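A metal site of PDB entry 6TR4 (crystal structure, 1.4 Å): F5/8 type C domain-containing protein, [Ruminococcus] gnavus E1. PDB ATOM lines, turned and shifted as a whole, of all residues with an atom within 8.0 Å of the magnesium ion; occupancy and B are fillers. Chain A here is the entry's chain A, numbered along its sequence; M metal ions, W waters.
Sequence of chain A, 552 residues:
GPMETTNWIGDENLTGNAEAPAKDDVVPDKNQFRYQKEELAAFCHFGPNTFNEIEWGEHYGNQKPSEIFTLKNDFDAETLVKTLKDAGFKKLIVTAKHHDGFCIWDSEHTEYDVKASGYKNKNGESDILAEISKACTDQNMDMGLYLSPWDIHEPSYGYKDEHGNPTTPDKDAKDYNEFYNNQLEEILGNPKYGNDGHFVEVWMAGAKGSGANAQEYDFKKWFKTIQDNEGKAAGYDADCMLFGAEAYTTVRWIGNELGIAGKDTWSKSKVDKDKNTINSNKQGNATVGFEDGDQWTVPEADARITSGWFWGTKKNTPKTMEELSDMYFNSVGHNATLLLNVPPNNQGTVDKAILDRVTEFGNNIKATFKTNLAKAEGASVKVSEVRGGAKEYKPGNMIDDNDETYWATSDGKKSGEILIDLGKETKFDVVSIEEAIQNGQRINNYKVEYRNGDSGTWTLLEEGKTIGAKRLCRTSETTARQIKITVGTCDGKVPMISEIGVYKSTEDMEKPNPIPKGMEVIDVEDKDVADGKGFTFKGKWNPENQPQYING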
ATOM      1  N   CYS A 103      14.752  -3.252 -22.392  1.00  0.00           N
ATOM      2  CA  CYS A 103      14.477  -1.882 -22.855  1.00  0.00           C
ATOM      3  C   CYS A 103      15.628  -0.954 -22.494  1.00  0.00           C
ATOM      4  O   CYS A 103      15.996  -0.865 -21.286  1.00  0.00           O
ATOM      5  CB  CYS A 103      13.153  -1.412 -22.281  1.00  0.00           C
ATOM      6  SG  CYS A 103      11.771  -2.408 -22.898  1.00  0.00           S
ATOM      7  N   TRP A 105      15.642   2.239 -22.603  1.00  0.00           N
ATOM      8  CA  TRP A 105      15.122   3.510 -22.047  1.00  0.00           C
ATOM      9  C   TRP A 105      14.500   3.200 -20.691  1.00  0.00           C
ATOM     10  O   TRP A 105      14.262   2.034 -20.394  1.00  0.00           O
ATOM     11  CB  TRP A 105      14.139   4.203 -22.992  1.00  0.00           C
ATOM     12  CG  TRP A 105      12.757   3.637 -22.960  1.00  0.00           C
ATOM     13  CD1 TRP A 105      11.668   4.182 -22.341  1.00  0.00           C
ATOM     14  CD2 TRP A 105      12.282   2.452 -23.645  1.00  0.00           C
ATOM     15  NE1 TRP A 105      10.576   3.400 -22.541  1.00  0.00           N
ATOM     16  CE2 TRP A 105      10.917   2.341 -23.353  1.00  0.00           C
ATOM     17  CE3 TRP A 105      12.868   1.496 -24.469  1.00  0.00           C
ATOM     18  CZ2 TRP A 105      10.127   1.286 -23.823  1.00  0.00           C
ATOM     19  CZ3 TRP A 105      12.099   0.447 -24.936  1.00  0.00           C
ATOM     20  CH2 TRP A 105      10.745   0.349 -24.610  1.00  0.00           C
ATOM     21  N   ASP A 106      14.274   4.227 -19.872  1.00  0.00           N
ATOM     22  CA  ASP A 106      13.687   4.047 -18.522  1.00  0.00           C
ATOM     23  C   ASP A 106      12.177   3.878 -18.680  1.00  0.00           C
ATOM     24  O   ASP A 106      11.475   4.892 -18.927  1.00  0.00           O
ATOM     25  CB  ASP A 106      14.083   5.249 -17.678  1.00  0.00           C
ATOM     26  CG  ASP A 106      13.565   5.241 -16.263  1.00  0.00           C
ATOM     27  OD1 ASP A 106      12.757   4.356 -15.943  1.00  0.00           O
ATOM     28  OD2 ASP A 106      13.983   6.145 -15.507  1.00  0.00           O
ATOM     29  N   SER A 107      11.675   2.643 -18.603  1.00  0.00           N
ATOM     30  CA  SER A 107      10.250   2.339 -18.898  1.00  0.00           C
ATOM     31  C   SER A 107       9.485   2.059 -17.621  1.00  0.00           C
ATOM     32  O   SER A 107       9.886   1.198 -16.839  1.00  0.00           O
ATOM     33  CB  SER A 107      10.110   1.170 -19.834  1.00  0.00           C
ATOM     34  OG  SER A 107       8.735   0.932 -20.083  1.00  0.00           O
ATOM     35  N   GLU A 108       8.358   2.741 -17.442  1.00  0.00           N
ATOM     36  CA  GLU A 108       7.451   2.469 -16.299  1.00  0.00           C
ATOM     37  C   GLU A 108       6.707   1.145 -16.524  1.00  0.00           C
ATOM     38  O   GLU A 108       6.188   0.614 -15.529  1.00  0.00           O
ATOM     39  CB  GLU A 108       6.497   3.658 -16.072  1.00  0.00           C
ATOM     40  CG  GLU A 108       5.477   3.881 -17.169  1.00  0.00           C
ATOM     41  CD  GLU A 108       4.595   5.109 -17.000  1.00  0.00           C
ATOM     42  OE1 GLU A 108       5.131   6.153 -16.566  1.00  0.00           O
ATOM     43  OE2 GLU A 108       3.371   5.006 -17.294  1.00  0.00           O
ATOM     44  N   HIS A 109       6.693   0.605 -17.753  1.00  0.00           N
ATOM     45  CA  HIS A 109       5.878  -0.592 -18.095  1.00  0.00           C
ATOM     46  C   HIS A 109       6.626  -1.895 -17.831  1.00  0.00           C
ATOM     47  O   HIS A 109       6.017  -2.959 -17.970  1.00  0.00           O
ATOM     48  CB  HIS A 109       5.416  -0.497 -19.547  1.00  0.00           C
ATOM     49  CG  HIS A 109       4.575   0.709 -19.755  1.00  0.00           C
ATOM     50  ND1 HIS A 109       3.317   0.826 -19.171  1.00  0.00           N
ATOM     51  CD2 HIS A 109       4.832   1.870 -20.386  1.00  0.00           C
ATOM     52  CE1 HIS A 109       2.846   2.017 -19.479  1.00  0.00           C
ATOM     53  NE2 HIS A 109       3.750   2.673 -20.234  1.00  0.00           N
ATOM     54  N   THR A 110       7.900  -1.833 -17.478  1.00  0.00           N
ATOM     55  CA  THR A 110       8.696  -3.042 -17.214  1.00  0.00           C
ATOM     56  C   THR A 110       9.843  -2.701 -16.278  1.00  0.00           C
ATOM     57  O   THR A 110      10.312  -1.557 -16.272  1.00  0.00           O
ATOM     58  CB  THR A 110       9.220  -3.666 -18.499  1.00  0.00           C
ATOM     59  OG1 THR A 110       9.911  -4.863 -18.141  1.00  0.00           O
ATOM     60  CG2 THR A 110      10.155  -2.744 -19.268  1.00  0.00           C
ATOM     61  N   GLU A 111      10.282  -3.691 -15.503  1.00  0.00           N
ATOM     62  CA  GLU A 111      11.523  -3.600 -14.701  1.00  0.00           C
ATOM     63  C   GLU A 111      12.673  -4.204 -15.507  1.00  0.00           C
ATOM     64  O   GLU A 111      13.777  -4.234 -14.991  1.00  0.00           O
ATOM     65  CB  GLU A 111      11.360  -4.288 -13.353  1.00  0.00           C
ATOM     66  CG  GLU A 111      10.355  -3.582 -12.447  1.00  0.00           C
ATOM     67  CD  GLU A 111      10.191  -4.213 -11.069  1.00  0.00           C
ATOM     68  OE1 GLU A 111      11.181  -4.725 -10.511  1.00  0.00           O
ATOM     69  OE2 GLU A 111       9.052  -4.188 -10.551  1.00  0.00           O
ATOM     70  N   TYR A 112      12.428  -4.673 -16.735  1.00  0.00           N
ATOM     71  CA  TYR A 112      13.483  -5.300 -17.553  1.00  0.00           C
ATOM     72  C   TYR A 112      14.099  -4.210 -18.427  1.00  0.00           C
ATOM     73  O   TYR A 112      13.900  -4.212 -19.657  1.00  0.00           O
ATOM     74  CB  TYR A 112      12.915  -6.470 -18.347  1.00  0.00           C
ATOM     75  CG  TYR A 112      13.902  -7.501 -18.799  1.00  0.00           C
ATOM     76  CD1 TYR A 112      14.599  -8.263 -17.882  1.00  0.00           C
ATOM     77  CD2 TYR A 112      14.039  -7.820 -20.141  1.00  0.00           C
ATOM     78  CE1 TYR A 112      15.454  -9.276 -18.303  1.00  0.00           C
ATOM     79  CE2 TYR A 112      14.875  -8.836 -20.585  1.00  0.00           C
ATOM     80  CZ  TYR A 112      15.575  -9.573 -19.642  1.00  0.00           C
ATOM     81  OH  TYR A 112      16.359 -10.630 -20.037  1.00  0.00           O
ATOM     82  N   ASP A 113      14.823  -3.286 -17.791  1.00  0.00           N
ATOM     83  CA  ASP A 113      15.276  -2.099 -18.532  1.00  0.00           C
ATOM     84  C   ASP A 113      16.575  -1.557 -17.946  1.00  0.00           C
ATOM     85  O   ASP A 113      17.110  -2.060 -16.930  1.00  0.00           O
ATOM     86  CB  ASP A 113      14.175  -1.029 -18.582  1.00  0.00           C
ATOM     87  CG  ASP A 113      13.773  -0.445 -17.253  1.00  0.00           C
ATOM     88  OD1 ASP A 113      14.569  -0.560 -16.302  1.00  0.00           O
ATOM     89  OD2 ASP A 113      12.670   0.115 -17.163  1.00  0.00           O
ATOM     90  N   VAL A 114      17.119  -0.563 -18.618  1.00  0.00           N
ATOM     91  CA  VAL A 114      18.446  -0.003 -18.271  1.00  0.00           C
ATOM     92  C   VAL A 114      18.377   0.681 -16.904  1.00  0.00           C
ATOM     93  O   VAL A 114      19.391   0.675 -16.199  1.00  0.00           O
ATOM     94  CB  VAL A 114      18.899   0.952 -19.385  1.00  0.00           C
ATOM     95  CG1 VAL A 114      17.894   2.083 -19.640  1.00  0.00           C
ATOM     96  CG2 VAL A 114      20.297   1.489 -19.096  1.00  0.00           C
ATOM     97  N   LYS A 115      17.216   1.205 -16.499  1.00  0.00           N
ATOM     98  CA  LYS A 115      17.115   1.825 -15.146  1.00  0.00           C
ATOM     99  C   LYS A 115      17.377   0.752 -14.075  1.00  0.00           C
ATOM    100  O   LYS A 115      18.148   1.001 -13.118  1.00  0.00           O
ATOM    101  CB  LYS A 115      15.756   2.472 -14.943  1.00  0.00           C
ATOM    102  CG  LYS A 115      15.555   3.153 -13.599  1.00  0.00           C
ATOM    103  CD  LYS A 115      16.222   4.501 -13.551  1.00  0.00           C
ATOM    104  CE  LYS A 115      15.656   5.422 -12.497  1.00  0.00           C
ATOM    105  NZ  LYS A 115      15.478   4.680 -11.231  1.00  0.00           N
ATOM    106  N   ALA A 116      16.844  -0.455 -14.241  1.00  0.00           N
ATOM    107  CA  ALA A 116      17.025  -1.558 -13.274  1.00  0.00           C
ATOM    108  C   ALA A 116      18.439  -2.138 -13.328  1.00  0.00           C
ATOM    109  O   ALA A 116      18.828  -2.849 -12.391  1.00  0.00           O
ATOM    110  CB  ALA A 116      16.004  -2.632 -13.525  1.00  0.00           C
ATOM    111  N   GLN A 183       4.251   1.125 -24.561  1.00  0.00           N
ATOM    112  CA  GLN A 183       5.683   1.471 -24.737  1.00  0.00           C
ATOM    113  C   GLN A 183       5.823   2.422 -25.922  1.00  0.00           C
ATOM    114  O   GLN A 183       6.646   3.356 -25.845  1.00  0.00           O
ATOM    115  CB  GLN A 183       6.534   0.216 -24.842  1.00  0.00           C
ATOM    116  CG  GLN A 183       6.664  -0.492 -23.500  1.00  0.00           C
ATOM    117  CD  GLN A 183       7.894  -1.352 -23.424  1.00  0.00           C
ATOM    118  OE1 GLN A 183       8.252  -2.047 -24.379  1.00  0.00           O
ATOM    119  NE2 GLN A 183       8.527  -1.341 -22.264  1.00  0.00           N
ATOM    120  N   GLU A 186       4.835   5.704 -24.563  1.00  0.00           N
ATOM    121  CA  GLU A 186       5.820   6.176 -23.569  1.00  0.00           C
ATOM    122  C   GLU A 186       7.006   6.827 -24.278  1.00  0.00           C
ATOM    123  O   GLU A 186       7.478   7.874 -23.799  1.00  0.00           O
ATOM    124  CB  GLU A 186       6.302   5.010 -22.717  1.00  0.00           C
ATOM    125  CG  GLU A 186       7.241   5.388 -21.612  1.00  0.00           C
ATOM    126  CD  GLU A 186       7.610   4.226 -20.729  1.00  0.00           C
ATOM    127  OE1 GLU A 186       7.966   3.169 -21.275  1.00  0.00           O
ATOM    128  OE2 GLU A 186       7.501   4.391 -19.471  1.00  0.00           O
HETATM  129 MG    MG M   1      11.205   0.263 -15.627  1.00  0.00          MG
HETATM  130  O   HOH W   1       9.872   0.146 -14.071  1.00  0.00           O
HETATM  131  O   HOH W   2      11.788   2.111 -15.006  1.00  0.00           O
HETATM  132  O   HOH W   3      12.735  -0.568 -14.399  1.00  0.00           O
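OG of Ser 107 is in hydrogen-bond range of N of His 109, at 3.1 Å.
OG of Ser 107 is in hydrogen-bond range of OE1 of Glu 186, at 2.6 Å.
The side-chain hydroxyl (OG) of Ser 107 sits at hydrogen-bond distance from the side-chain amide nitrogen (NE2) of Gln 183, 3.2 Å away.
N of Tyr 112 lies within hydrogen-bond range of OG1 of Thr 110, 2.9 Å away.
OD1 of Asp 113 sits close to N of Lys 115 (3.2 Å).
OD1 of Asp 113 lies within hydrogen-bond range of N of Ala 116 (3.1 Å).
Merely in contact with the magnesium ion: Glu 111 (3.99 Å).
Of the 15 residues printed, 4 come within 4 Å of the magnesium ion.
O of Ser 107 is bound to the magnesium ion, 2.0 Å away.
The magnesium ion is bound by water W2 (2.0 Å).
Water W1 is bound to the magnesium ion (2.1 Å).
The magnesium ion is bound by the backbone carbonyl oxygen (O) of Thr 110, at 2.1 Å.
The magnesium ion is bound by OD2 of Asp 113, at 2.1 Å.
The magnesium ion is bound by water W3 (2.1 Å).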
